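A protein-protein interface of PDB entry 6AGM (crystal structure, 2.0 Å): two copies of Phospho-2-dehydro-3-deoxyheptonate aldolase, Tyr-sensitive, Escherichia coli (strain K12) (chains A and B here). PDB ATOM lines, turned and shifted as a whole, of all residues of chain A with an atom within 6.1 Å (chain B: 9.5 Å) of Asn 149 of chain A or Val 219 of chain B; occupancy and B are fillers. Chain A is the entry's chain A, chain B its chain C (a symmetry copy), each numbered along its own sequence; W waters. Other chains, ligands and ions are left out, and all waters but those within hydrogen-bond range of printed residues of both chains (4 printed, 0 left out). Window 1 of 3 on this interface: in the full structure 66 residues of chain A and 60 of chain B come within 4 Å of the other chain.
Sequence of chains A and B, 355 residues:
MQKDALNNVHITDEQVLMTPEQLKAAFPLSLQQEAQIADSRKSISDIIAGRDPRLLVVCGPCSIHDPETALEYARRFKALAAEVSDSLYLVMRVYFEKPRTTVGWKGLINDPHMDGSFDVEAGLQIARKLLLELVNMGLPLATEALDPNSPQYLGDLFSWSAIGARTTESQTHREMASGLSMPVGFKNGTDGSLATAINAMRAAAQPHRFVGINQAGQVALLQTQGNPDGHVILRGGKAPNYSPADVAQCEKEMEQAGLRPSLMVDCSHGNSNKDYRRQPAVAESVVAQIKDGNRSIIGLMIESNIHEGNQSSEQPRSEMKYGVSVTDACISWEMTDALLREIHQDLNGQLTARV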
ATOM      1  N   GLN A  15     -26.116   1.116  25.367  1.00  0.00           N
ATOM      2  CA  GLN A  15     -24.775   0.550  25.376  1.00  0.00           C
ATOM      3  C   GLN A  15     -23.943   1.168  24.261  1.00  0.00           C
ATOM      4  O   GLN A  15     -24.457   1.474  23.181  1.00  0.00           O
ATOM      5  CB  GLN A  15     -24.812  -0.981  25.241  1.00  0.00           C
ATOM      6  CG  GLN A  15     -25.011  -1.503  23.833  1.00  0.00           C
ATOM      7  CD  GLN A  15     -24.587  -2.952  23.691  1.00  0.00           C
ATOM      8  OE1 GLN A  15     -25.156  -3.843  24.323  1.00  0.00           O
ATOM      9  NE2 GLN A  15     -23.578  -3.196  22.860  1.00  0.00           N
ATOM     10  N   VAL A  16     -22.654   1.361  24.540  1.00  0.00           N
ATOM     11  CA  VAL A  16     -21.752   1.969  23.571  1.00  0.00           C
ATOM     12  C   VAL A  16     -21.446   0.967  22.467  1.00  0.00           C
ATOM     13  O   VAL A  16     -21.033  -0.170  22.731  1.00  0.00           O
ATOM     14  CB  VAL A  16     -20.471   2.457  24.265  1.00  0.00           C
ATOM     15  CG1 VAL A  16     -19.523   3.107  23.266  1.00  0.00           C
ATOM     16  CG2 VAL A  16     -20.817   3.432  25.378  1.00  0.00           C
ATOM     17  N   LEU A  17     -21.655   1.379  21.224  1.00  0.00           N
ATOM     18  CA  LEU A  17     -21.398   0.505  20.093  1.00  0.00           C
ATOM     19  C   LEU A  17     -19.900   0.384  19.836  1.00  0.00           C
ATOM     20  O   LEU A  17     -19.120   1.294  20.133  1.00  0.00           O
ATOM     21  CB  LEU A  17     -22.108   1.031  18.846  1.00  0.00           C
ATOM     22  CG  LEU A  17     -22.222   0.092  17.647  1.00  0.00           C
ATOM     23  CD1 LEU A  17     -23.240  -1.003  17.921  1.00  0.00           C
ATOM     24  CD2 LEU A  17     -22.592   0.879  16.395  1.00  0.00           C
ATOM     25  N   MET A  18     -19.502  -0.768  19.301  1.00  0.00           N
ATOM     26  CA  MET A  18     -18.132  -0.961  18.844  1.00  0.00           C
ATOM     27  C   MET A  18     -17.738   0.158  17.886  1.00  0.00           C
ATOM     28  O   MET A  18     -18.513   0.536  17.005  1.00  0.00           O
ATOM     29  CB  MET A  18     -18.008  -2.328  18.165  1.00  0.00           C
ATOM     30  CG  MET A  18     -16.774  -2.524  17.300  1.00  0.00           C
ATOM     31  SD  MET A  18     -16.837  -4.107  16.428  1.00  0.00           S
ATOM     32  CE  MET A  18     -16.656  -5.258  17.792  1.00  0.00           C
ATOM     33  N   PRO A  20     -15.400   2.285  14.984  1.00  0.00           N
ATOM     34  CA  PRO A  20     -14.682   1.941  13.743  1.00  0.00           C
ATOM     35  C   PRO A  20     -13.271   1.440  13.988  1.00  0.00           C
ATOM     36  O   PRO A  20     -12.826   0.495  13.322  1.00  0.00           O
ATOM     37  CB  PRO A  20     -14.687   3.263  12.961  1.00  0.00           C
ATOM     38  CG  PRO A  20     -15.898   3.983  13.451  1.00  0.00           C
ATOM     39  CD  PRO A  20     -16.044   3.611  14.903  1.00  0.00           C
ATOM     40  N   ASP A 147     -25.492   7.925   5.236  1.00  0.00           N
ATOM     41  CA  ASP A 147     -25.289   8.039   6.670  1.00  0.00           C
ATOM     42  C   ASP A 147     -23.873   8.525   6.917  1.00  0.00           C
ATOM     43  O   ASP A 147     -22.960   8.107   6.193  1.00  0.00           O
ATOM     44  CB  ASP A 147     -25.524   6.676   7.335  1.00  0.00           C
ATOM     45  CG  ASP A 147     -25.332   6.710   8.825  1.00  0.00           C
ATOM     46  OD1 ASP A 147     -24.168   6.658   9.268  1.00  0.00           O
ATOM     47  OD2 ASP A 147     -26.345   6.770   9.555  1.00  0.00           O
ATOM     48  N   PRO A 148     -23.644   9.402   7.900  1.00  0.00           N
ATOM     49  CA  PRO A 148     -22.283   9.905   8.138  1.00  0.00           C
ATOM     50  C   PRO A 148     -21.381   8.947   8.901  1.00  0.00           C
ATOM     51  O   PRO A 148     -20.178   9.221   9.008  1.00  0.00           O
ATOM     52  CB  PRO A 148     -22.517  11.191   8.954  1.00  0.00           C
ATOM     53  CG  PRO A 148     -24.009  11.429   8.935  1.00  0.00           C
ATOM     54  CD  PRO A 148     -24.636  10.091   8.738  1.00  0.00           C
ATOM     55  N   ASN A 149     -21.911   7.845   9.433  1.00  0.00           N
ATOM     56  CA  ASN A 149     -21.133   6.928  10.259  1.00  0.00           C
ATOM     57  C   ASN A 149     -20.663   5.691   9.507  1.00  0.00           C
ATOM     58  O   ASN A 149     -19.542   5.228   9.732  1.00  0.00           O
ATOM     59  CB  ASN A 149     -21.948   6.492  11.482  1.00  0.00           C
ATOM     60  CG  ASN A 149     -22.493   7.668  12.271  1.00  0.00           C
ATOM     61  OD1 ASN A 149     -22.282   8.826  11.910  1.00  0.00           O
ATOM     62  ND2 ASN A 149     -23.207   7.375  13.351  1.00  0.00           N
ATOM     63  N   SER A 150     -21.495   5.137   8.625  1.00  0.00           N
ATOM     64  CA  SER A 150     -21.104   3.929   7.908  1.00  0.00           C
ATOM     65  C   SER A 150     -19.835   4.082   7.069  1.00  0.00           C
ATOM     66  O   SER A 150     -19.117   3.077   6.921  1.00  0.00           O
ATOM     67  CB  SER A 150     -22.274   3.443   7.036  1.00  0.00           C
ATOM     68  OG  SER A 150     -23.007   4.533   6.505  1.00  0.00           O
ATOM     69  N   PRO A 151     -19.509   5.248   6.490  1.00  0.00           N
ATOM     70  CA  PRO A 151     -18.192   5.367   5.846  1.00  0.00           C
ATOM     71  C   PRO A 151     -17.037   5.137   6.804  1.00  0.00           C
ATOM     72  O   PRO A 151     -16.076   4.471   6.419  1.00  0.00           O
ATOM     73  CB  PRO A 151     -18.210   6.793   5.280  1.00  0.00           C
ATOM     74  CG  PRO A 151     -19.639   7.047   5.005  1.00  0.00           C
ATOM     75  CD  PRO A 151     -20.370   6.395   6.144  1.00  0.00           C
ATOM     76  N   GLN A 152     -17.137   5.578   8.057  1.00  0.00           N
ATOM     77  CA  GLN A 152     -16.049   5.322   8.996  1.00  0.00           C
ATOM     78  C   GLN A 152     -15.893   3.834   9.274  1.00  0.00           C
ATOM     79  O   GLN A 152     -14.771   3.346   9.457  1.00  0.00           O
ATOM     80  CB  GLN A 152     -16.284   6.086  10.297  1.00  0.00           C
ATOM     81  CG  GLN A 152     -16.066   7.579  10.181  1.00  0.00           C
ATOM     82  CD  GLN A 152     -14.594   7.952  10.121  1.00  0.00           C
ATOM     83  OE1 GLN A 152     -13.871   7.534   9.215  1.00  0.00           O
ATOM     84  NE2 GLN A 152     -14.145   8.740  11.091  1.00  0.00           N
ATOM     85  N   TYR A 153     -17.004   3.095   9.310  1.00  0.00           N
ATOM     86  CA  TYR A 153     -16.938   1.676   9.634  1.00  0.00           C
ATOM     87  C   TYR A 153     -16.455   0.842   8.453  1.00  0.00           C
ATOM     88  O   TYR A 153     -15.657  -0.084   8.636  1.00  0.00           O
ATOM     89  CB  TYR A 153     -18.308   1.179  10.105  1.00  0.00           C
ATOM     90  CG  TYR A 153     -18.661   1.614  11.512  1.00  0.00           C
ATOM     91  CD1 TYR A 153     -19.423   2.752  11.739  1.00  0.00           C
ATOM     92  CD2 TYR A 153     -18.227   0.888  12.613  1.00  0.00           C
ATOM     93  CE1 TYR A 153     -19.745   3.155  13.025  1.00  0.00           C
ATOM     94  CE2 TYR A 153     -18.543   1.281  13.902  1.00  0.00           C
ATOM     95  CZ  TYR A 153     -19.302   2.416  14.101  1.00  0.00           C
ATOM     96  OH  TYR A 153     -19.617   2.808  15.382  1.00  0.00           O
ATOM     97  N   LEU A 154     -16.921   1.143   7.234  1.00  0.00           N
ATOM     98  CA  LEU A 154     -16.690   0.240   6.112  1.00  0.00           C
ATOM     99  C   LEU A 154     -16.186   0.886   4.824  1.00  0.00           C
ATOM    100  O   LEU A 154     -15.917   0.155   3.864  1.00  0.00           O
ATOM    101  CB  LEU A 154     -17.978  -0.536   5.791  1.00  0.00           C
ATOM    102  CG  LEU A 154     -18.628  -1.325   6.930  1.00  0.00           C
ATOM    103  CD1 LEU A 154     -19.951  -1.921   6.473  1.00  0.00           C
ATOM    104  CD2 LEU A 154     -17.696  -2.412   7.443  1.00  0.00           C
ATOM    105  N   MET A 176     -20.508  15.949   2.895  1.00  0.00           N
ATOM    106  CA  MET A 176     -19.708  14.782   3.247  1.00  0.00           C
ATOM    107  C   MET A 176     -18.908  14.262   2.058  1.00  0.00           C
ATOM    108  O   MET A 176     -17.795  13.756   2.237  1.00  0.00           O
ATOM    109  CB  MET A 176     -20.607  13.683   3.811  1.00  0.00           C
ATOM    110  CG  MET A 176     -19.835  12.485   4.329  1.00  0.00           C
ATOM    111  SD  MET A 176     -20.907  11.236   5.051  1.00  0.00           S
ATOM    112  CE  MET A 176     -21.962  10.853   3.655  1.00  0.00           C
ATOM    113  N   GLY A 212     -19.713  14.397  11.603  1.00  0.00           N
ATOM    114  CA  GLY A 212     -19.737  12.941  11.518  1.00  0.00           C
ATOM    115  C   GLY A 212     -19.211  12.347  12.794  1.00  0.00           C
ATOM    116  O   GLY A 212     -19.491  12.859  13.887  1.00  0.00           O
ATOM    117  N   ILE A 213     -18.424  11.282  12.675  1.00  0.00           N
ATOM    118  CA  ILE A 213     -17.773  10.677  13.828  1.00  0.00           C
ATOM    119  C   ILE A 213     -16.305  10.447  13.501  1.00  0.00           C
ATOM    120  O   ILE A 213     -15.922  10.312  12.333  1.00  0.00           O
ATOM    121  CB  ILE A 213     -18.445   9.351  14.259  1.00  0.00           C
ATOM    122  CG1 ILE A 213     -18.369   8.311  13.139  1.00  0.00           C
ATOM    123  CG2 ILE A 213     -19.888   9.587  14.694  1.00  0.00           C
ATOM    124  CD1 ILE A 213     -18.790   6.915  13.579  1.00  0.00           C
ATOM    125  N   ALA A 216     -12.941   6.833  16.846  1.00  0.00           N
ATOM    126  CA  ALA A 216     -13.308   6.399  18.187  1.00  0.00           C
ATOM    127  C   ALA A 216     -14.808   6.505  18.445  1.00  0.00           C
ATOM    128  O   ALA A 216     -15.235   6.466  19.604  1.00  0.00           O
ATOM    129  CB  ALA A 216     -12.534   7.203  19.236  1.00  0.00           C
ATOM    130  N   GLY A 217     -15.612   6.659  17.394  1.00  0.00           N
ATOM    131  CA  GLY A 217     -17.051   6.687  17.553  1.00  0.00           C
ATOM    132  C   GLY A 217     -17.602   7.922  18.222  1.00  0.00           C
ATOM    133  O   GLY A 217     -18.743   7.900  18.691  1.00  0.00           O
ATOM    134  N   GLN A 218     -16.833   9.005  18.276  1.00  0.00           N
ATOM    135  CA  GLN A 218     -17.263  10.238  18.921  1.00  0.00           C
ATOM    136  C   GLN A 218     -17.773  11.225  17.881  1.00  0.00           C
ATOM    137  O   GLN A 218     -17.206  11.342  16.791  1.00  0.00           O
ATOM    138  CB  GLN A 218     -16.119  10.875  19.713  1.00  0.00           C
ATOM    139  CG  GLN A 218     -15.539   9.996  20.803  1.00  0.00           C
ATOM    140  CD  GLN A 218     -14.307  10.610  21.442  1.00  0.00           C
ATOM    141  OE1 GLN A 218     -13.240  10.662  20.833  1.00  0.00           O
ATOM    142  NE2 GLN A 218     -14.455  11.086  22.672  1.00  0.00           N
ATOM    143  N   VAL A 219     -18.849  11.937  18.228  1.00  0.00           N
ATOM    144  CA  VAL A 219     -19.352  12.994  17.361  1.00  0.00           C
ATOM    145  C   VAL A 219     -18.252  14.018  17.139  1.00  0.00           C
ATOM    146  O   VAL A 219     -17.652  14.525  18.094  1.00  0.00           O
ATOM    147  CB  VAL A 219     -20.607  13.635  17.970  1.00  0.00           C
ATOM    148  CG1 VAL A 219     -21.179  14.683  17.024  1.00  0.00           C
ATOM    149  CG2 VAL A 219     -21.646  12.568  18.275  1.00  0.00           C
ATOM    150  N   PRO B  20     -23.341  16.191  24.608  1.00  0.00           N
ATOM    151  CA  PRO B  20     -24.566  16.566  25.341  1.00  0.00           C
ATOM    152  C   PRO B  20     -24.332  16.782  26.828  1.00  0.00           C
ATOM    153  O   PRO B  20     -24.895  17.719  27.415  1.00  0.00           O
ATOM    154  CB  PRO B  20     -25.502  15.377  25.077  1.00  0.00           C
ATOM    155  CG  PRO B  20     -25.044  14.830  23.762  1.00  0.00           C
ATOM    156  CD  PRO B  20     -23.553  15.031  23.723  1.00  0.00           C
ATOM    157  N   ASP B 147     -32.577  13.944  13.108  1.00  0.00           N
ATOM    158  CA  ASP B 147     -31.348  13.183  13.286  1.00  0.00           C
ATOM    159  C   ASP B 147     -31.315  12.667  14.718  1.00  0.00           C
ATOM    160  O   ASP B 147     -32.054  13.165  15.574  1.00  0.00           O
ATOM    161  CB  ASP B 147     -30.113  14.051  12.987  1.00  0.00           C
ATOM    162  CG  ASP B 147     -30.016  15.256  13.896  1.00  0.00           C
ATOM    163  OD1 ASP B 147     -29.525  15.101  15.037  1.00  0.00           O
ATOM    164  OD2 ASP B 147     -30.431  16.355  13.477  1.00  0.00           O
ATOM    165  N   PRO B 148     -30.485  11.662  15.007  1.00  0.00           N
ATOM    166  CA  PRO B 148     -30.434  11.115  16.371  1.00  0.00           C
ATOM    167  C   PRO B 148     -29.565  11.905  17.339  1.00  0.00           C
ATOM    168  O   PRO B 148     -29.464  11.514  18.507  1.00  0.00           O
ATOM    169  CB  PRO B 148     -29.858   9.699  16.159  1.00  0.00           C
ATOM    170  CG  PRO B 148     -29.821   9.484  14.666  1.00  0.00           C
ATOM    171  CD  PRO B 148     -29.710  10.839  14.066  1.00  0.00           C
ATOM    172  N   ASN B 149     -28.940  12.996  16.902  1.00  0.00           N
ATOM    173  CA  ASN B 149     -28.034  13.748  17.761  1.00  0.00           C
ATOM    174  C   ASN B 149     -28.737  14.890  18.486  1.00  0.00           C
ATOM    175  O   ASN B 149     -28.598  15.032  19.705  1.00  0.00           O
ATOM    176  CB  ASN B 149     -26.862  14.296  16.938  1.00  0.00           C
ATOM    177  CG  ASN B 149     -25.898  13.213  16.504  1.00  0.00           C
ATOM    178  OD1 ASN B 149     -26.136  12.028  16.726  1.00  0.00           O
ATOM    179  ND2 ASN B 149     -24.799  13.616  15.874  1.00  0.00           N
ATOM    180  N   GLN B 152     -30.466  14.431  21.866  1.00  0.00           N
ATOM    181  CA  GLN B 152     -29.618  14.346  23.050  1.00  0.00           C
ATOM    182  C   GLN B 152     -29.132  15.717  23.505  1.00  0.00           C
ATOM    183  O   GLN B 152     -28.948  15.938  24.707  1.00  0.00           O
ATOM    184  CB  GLN B 152     -28.431  13.422  22.785  1.00  0.00           C
ATOM    185  CG  GLN B 152     -28.811  11.955  22.717  1.00  0.00           C
ATOM    186  CD  GLN B 152     -29.106  11.353  24.084  1.00  0.00           C
ATOM    187  OE1 GLN B 152     -29.989  11.816  24.806  1.00  0.00           O
ATOM    188  NE2 GLN B 152     -28.370  10.304  24.439  1.00  0.00           N
ATOM    189  N   THR B 172     -30.846   2.988  10.537  1.00  0.00           N
ATOM    190  CA  THR B 172     -30.147   3.065  11.812  1.00  0.00           C
ATOM    191  C   THR B 172     -31.068   3.517  12.941  1.00  0.00           C
ATOM    192  O   THR B 172     -30.937   3.032  14.070  1.00  0.00           O
ATOM    193  CB  THR B 172     -28.955   4.016  11.693  1.00  0.00           C
ATOM    194  OG1 THR B 172     -29.313   5.129  10.868  1.00  0.00           O
ATOM    195  CG2 THR B 172     -27.767   3.300  11.081  1.00  0.00           C
ATOM    196  N   HIS B 173     -32.018   4.420  12.660  1.00  0.00           N
ATOM    197  CA  HIS B 173     -32.796   5.031  13.732  1.00  0.00           C
ATOM    198  C   HIS B 173     -34.260   5.233  13.342  1.00  0.00           C
ATOM    199  O   HIS B 173     -34.897   6.193  13.792  1.00  0.00           O
ATOM    200  CB  HIS B 173     -32.175   6.369  14.149  1.00  0.00           C
ATOM    201  CG  HIS B 173     -31.785   7.238  12.993  1.00  0.00           C
ATOM    202  ND1 HIS B 173     -30.657   7.013  12.235  1.00  0.00           N
ATOM    203  CD2 HIS B 173     -32.380   8.334  12.466  1.00  0.00           C
ATOM    204  CE1 HIS B 173     -30.573   7.931  11.289  1.00  0.00           C
ATOM    205  NE2 HIS B 173     -31.606   8.746  11.408  1.00  0.00           N
ATOM    206  N   PHE B 210     -32.565   1.443  18.433  1.00  0.00           N
ATOM    207  CA  PHE B 210     -32.068   2.303  17.363  1.00  0.00           C
ATOM    208  C   PHE B 210     -30.645   2.744  17.674  1.00  0.00           C
ATOM    209  O   PHE B 210     -30.182   2.666  18.813  1.00  0.00           O
ATOM    210  CB  PHE B 210     -32.992   3.513  17.125  1.00  0.00           C
ATOM    211  CG  PHE B 210     -32.927   4.571  18.199  1.00  0.00           C
ATOM    212  CD1 PHE B 210     -32.086   5.665  18.066  1.00  0.00           C
ATOM    213  CD2 PHE B 210     -33.736   4.492  19.321  1.00  0.00           C
ATOM    214  CE1 PHE B 210     -32.031   6.647  19.047  1.00  0.00           C
ATOM    215  CE2 PHE B 210     -33.691   5.469  20.302  1.00  0.00           C
ATOM    216  CZ  PHE B 210     -32.836   6.550  20.162  1.00  0.00           C
ATOM    217  N   VAL B 211     -29.947   3.195  16.637  1.00  0.00           N
ATOM    218  CA  VAL B 211     -28.582   3.695  16.777  1.00  0.00           C
ATOM    219  C   VAL B 211     -28.638   5.207  16.956  1.00  0.00           C
ATOM    220  O   VAL B 211     -29.176   5.923  16.106  1.00  0.00           O
ATOM    221  CB  VAL B 211     -27.718   3.321  15.564  1.00  0.00           C
ATOM    222  CG1 VAL B 211     -26.314   3.891  15.719  1.00  0.00           C
ATOM    223  CG2 VAL B 211     -27.675   1.810  15.385  1.00  0.00           C
ATOM    224  N   GLY B 212     -28.083   5.690  18.064  1.00  0.00           N
ATOM    225  CA  GLY B 212     -27.968   7.116  18.295  1.00  0.00           C
ATOM    226  C   GLY B 212     -26.657   7.441  18.974  1.00  0.00           C
ATOM    227  O   GLY B 212     -25.629   6.829  18.669  1.00  0.00           O
ATOM    228  N   ILE B 213     -26.671   8.384  19.914  1.00  0.00           N
ATOM    229  CA  ILE B 213     -25.493   8.682  20.715  1.00  0.00           C
ATOM    230  C   ILE B 213     -25.891   8.686  22.183  1.00  0.00           C
ATOM    231  O   ILE B 213     -27.058   8.875  22.536  1.00  0.00           O
ATOM    232  CB  ILE B 213     -24.834  10.028  20.335  1.00  0.00           C
ATOM    233  CG1 ILE B 213     -25.783  11.193  20.617  1.00  0.00           C
ATOM    234  CG2 ILE B 213     -24.404  10.019  18.877  1.00  0.00           C
ATOM    235  CD1 ILE B 213     -25.186  12.553  20.328  1.00  0.00           C
ATOM    236  N   ASN B 214     -24.899   8.467  23.046  1.00  0.00           N
ATOM    237  CA  ASN B 214     -25.133   8.627  24.469  1.00  0.00           C
ATOM    238  C   ASN B 214     -24.800  10.061  24.872  1.00  0.00           C
ATOM    239  O   ASN B 214     -24.426  10.897  24.044  1.00  0.00           O
ATOM    240  CB  ASN B 214     -24.345   7.591  25.280  1.00  0.00           C
ATOM    241  CG  ASN B 214     -22.831   7.736  25.152  1.00  0.00           C
ATOM    242  OD1 ASN B 214     -22.314   8.739  24.664  1.00  0.00           O
ATOM    243  ND2 ASN B 214     -22.113   6.719  25.618  1.00  0.00           N
ATOM    244  N   GLN B 215     -24.941  10.352  26.165  1.00  0.00           N
ATOM    245  CA  GLN B 215     -24.680  11.698  26.657  1.00  0.00           C
ATOM    246  C   GLN B 215     -23.212  12.089  26.533  1.00  0.00           C
ATOM    247  O   GLN B 215     -22.891  13.279  26.619  1.00  0.00           O
ATOM    248  CB  GLN B 215     -25.141  11.820  28.109  1.00  0.00           C
ATOM    249  CG  GLN B 215     -26.645  12.006  28.253  1.00  0.00           C
ATOM    250  CD  GLN B 215     -27.118  13.341  27.709  1.00  0.00           C
ATOM    251  OE1 GLN B 215     -26.681  14.399  28.163  1.00  0.00           O
ATOM    252  NE2 GLN B 215     -28.012  13.298  26.727  1.00  0.00           N
ATOM    253  N   ALA B 216     -22.319  11.123  26.331  1.00  0.00           N
ATOM    254  CA  ALA B 216     -20.905  11.400  26.121  1.00  0.00           C
ATOM    255  C   ALA B 216     -20.548  11.565  24.647  1.00  0.00           C
ATOM    256  O   ALA B 216     -19.362  11.592  24.309  1.00  0.00           O
ATOM    257  CB  ALA B 216     -20.052  10.290  26.741  1.00  0.00           C
ATOM    258  N   GLY B 217     -21.543  11.663  23.766  1.00  0.00           N
ATOM    259  CA  GLY B 217     -21.275  11.838  22.352  1.00  0.00           C
ATOM    260  C   GLY B 217     -20.713  10.626  21.645  1.00  0.00           C
ATOM    261  O   GLY B 217     -20.068  10.774  20.604  1.00  0.00           O
ATOM    262  N   GLN B 218     -20.933   9.427  22.177  1.00  0.00           N
ATOM    263  CA  GLN B 218     -20.453   8.195  21.567  1.00  0.00           C
ATOM    264  C   GLN B 218     -21.594   7.494  20.845  1.00  0.00           C
ATOM    265  O   GLN B 218     -22.725   7.474  21.336  1.00  0.00           O
ATOM    266  CB  GLN B 218     -19.865   7.253  22.618  1.00  0.00           C
ATOM    267  CG  GLN B 218     -18.674   7.815  23.369  1.00  0.00           C
ATOM    268  CD  GLN B 218     -18.349   7.003  24.604  1.00  0.00           C
ATOM    269  OE1 GLN B 218     -19.137   6.947  25.548  1.00  0.00           O
ATOM    270  NE2 GLN B 218     -17.185   6.359  24.600  1.00  0.00           N
ATOM    271  N   VAL B 219     -21.288   6.920  19.678  1.00  0.00           N
ATOM    272  CA  VAL B 219     -22.264   6.099  18.973  1.00  0.00           C
ATOM    273  C   VAL B 219     -22.728   4.984  19.898  1.00  0.00           C
ATOM    274  O   VAL B 219     -21.915   4.259  20.486  1.00  0.00           O
ATOM    275  CB  VAL B 219     -21.666   5.543  17.671  1.00  0.00           C
ATOM    276  CG1 VAL B 219     -22.650   4.598  16.990  1.00  0.00           C
ATOM    277  CG2 VAL B 219     -21.284   6.678  16.730  1.00  0.00           C
ATOM    278  N   ALA B 220     -24.044   4.855  20.047  1.00  0.00           N
ATOM    279  CA  ALA B 220     -24.621   3.966  21.041  1.00  0.00           C
ATOM    280  C   ALA B 220     -25.845   3.269  20.469  1.00  0.00           C
ATOM    281  O   ALA B 220     -26.506   3.776  19.559  1.00  0.00           O
ATOM    282  CB  ALA B 220     -25.008   4.727  22.319  1.00  0.00           C
ATOM    283  N   LEU B 221     -26.129   2.087  21.007  1.00  0.00           N
ATOM    284  CA  LEU B 221     -27.344   1.352  20.696  1.00  0.00           C
ATOM    285  C   LEU B 221     -28.320   1.551  21.845  1.00  0.00           C
ATOM    286  O   LEU B 221     -27.997   1.245  22.999  1.00  0.00           O
ATOM    287  CB  LEU B 221     -27.050  -0.132  20.480  1.00  0.00           C
ATOM    288  CG  LEU B 221     -28.263  -0.970  20.076  1.00  0.00           C
ATOM    289  CD1 LEU B 221     -28.804  -0.451  18.765  1.00  0.00           C
ATOM    290  CD2 LEU B 221     -27.900  -2.444  19.962  1.00  0.00           C
ATOM    291  N   LEU B 222     -29.503   2.072  21.539  1.00  0.00           N
ATOM    292  CA  LEU B 222     -30.486   2.433  22.545  1.00  0.00           C
ATOM    293  C   LEU B 222     -31.693   1.515  22.439  1.00  0.00           C
ATOM    294  O   LEU B 222     -32.223   1.296  21.343  1.00  0.00           O
ATOM    295  CB  LEU B 222     -30.906   3.894  22.390  1.00  0.00           C
ATOM    296  CG  LEU B 222     -29.719   4.838  22.592  1.00  0.00           C
ATOM    297  CD1 LEU B 222     -29.523   5.713  21.376  1.00  0.00           C
ATOM    298  CD2 LEU B 222     -29.889   5.674  23.852  1.00  0.00           C
HETATM  299  O   HOH W   1     -25.335   7.844  15.810  1.00  0.00           O
HETATM  300  O   HOH W   2     -17.239  12.477  22.577  1.00  0.00           O
HETATM  301  O   HOH W   3     -17.401   5.526  21.343  1.00  0.00           O
HETATM  302  O   HOH W   4     -19.243   4.055  19.787  1.00  0.00           O
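The backbone carbonyl oxygen (O) of Gln 15 of chain A sits at hydrogen-bond distance from the backbone NH (N) of Leu 221 of chain B (2.8 Å).
The backbone carbonyl oxygen (O) of Val 219 of chain B lies within hydrogen-bond range of the backbone NH (N) of Leu 17 of chain A (3.0 Å).
The backbone carbonyl oxygen (O) of Gly 217 of chain A is in hydrogen-bond range of the backbone NH (N) of Val 219 of chain B, at 2.9 Å.
O of Gly 217 of chain B is in hydrogen-bond range of N of Val 219 of chain A (2.9 Å).
OD1 of Asp 147 of chain A sits at hydrogen-bond distance from N of Asn 149 of chain A.
The side-chain amide nitrogen (NE2) of Gln 152 of chain A sits at hydrogen-bond distance from the backbone carbonyl oxygen (O) of Ile 213 of chain A.
CG1 of Val 219 of chain B touches OH of Tyr 153 of chain A, at 3.9 Å.
O of Gly 217 of chain A touches O of Gly 217 of chain B (3.7 Å).
O of Gly 217 of chain B touches CA of Gln 218 of chain A, 3.3 Å away.
Val 219 of chain A touches Ile 213 of chain B.
Val 16 of chain A touches three residues of chain B.
Pro 148 of chain A touches none of the printed residues of chain B.
Asn 149 of chain A touches just one residue of chain B: Val 219 (3.9 Å).
No residue of chain B comes within 4 Å of Ser 150 of chain A.
No residue of chain B comes within 4 Å of Pro 151 of chain A.
Ala 216 of chain A touches none of the printed residues of chain B.
Of the printed residues of chain B, Gly 217 of chain A touches Gly 217 (3.7 Å), Gln 218 (3.4 Å) and Val 219 (2.9 Å).
The nearest residue of chain B that does not touch Asn 149 of chain A is Val 211 of chain B (5.2 Å).
The nearest residue of chain A that does not touch Val 219 of chain B is Gln 15 of chain A (4.6 Å).
The nearest printed residue of chain A that does not touch Thr 172 of chain B is Asn 149 of chain A (6.5 Å).
Of the 20 printed residues of chain B, 9 touch a printed residue of chain A.
Printed residues of chain B that touch a printed residue of chain A: Asn 149, Thr 172, Ile 213, Asn 214, Gly 217, Gln 218, Val 219, Ala 220 and Leu 221.
Hydrophobic or aromatic side chains of chain B within 4 Å of the printed part of chain A: Ile 213, Val 219 and Ala 220.
Among the printed residues, no Asp or Glu carboxylate lies within 4 Å of a Lys or Arg side-chain nitrogen of the other chain.
Asn 149 of chain A touches Val 219 of chain B, and with the chains exchanged Val 219 of chain A touches Asn 149 of chain B.
Ile 213 of chain A touches Val 219 of chain B, and with the chains exchanged Val 219 of chain A touches Ile 213 of chain B.
Water W1 bridges the backbone carbonyl oxygen of Gly 212 of chain B (3.0 Å) and the side-chain amide nitrogen of Asn 149 of chain A (3.3 Å).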
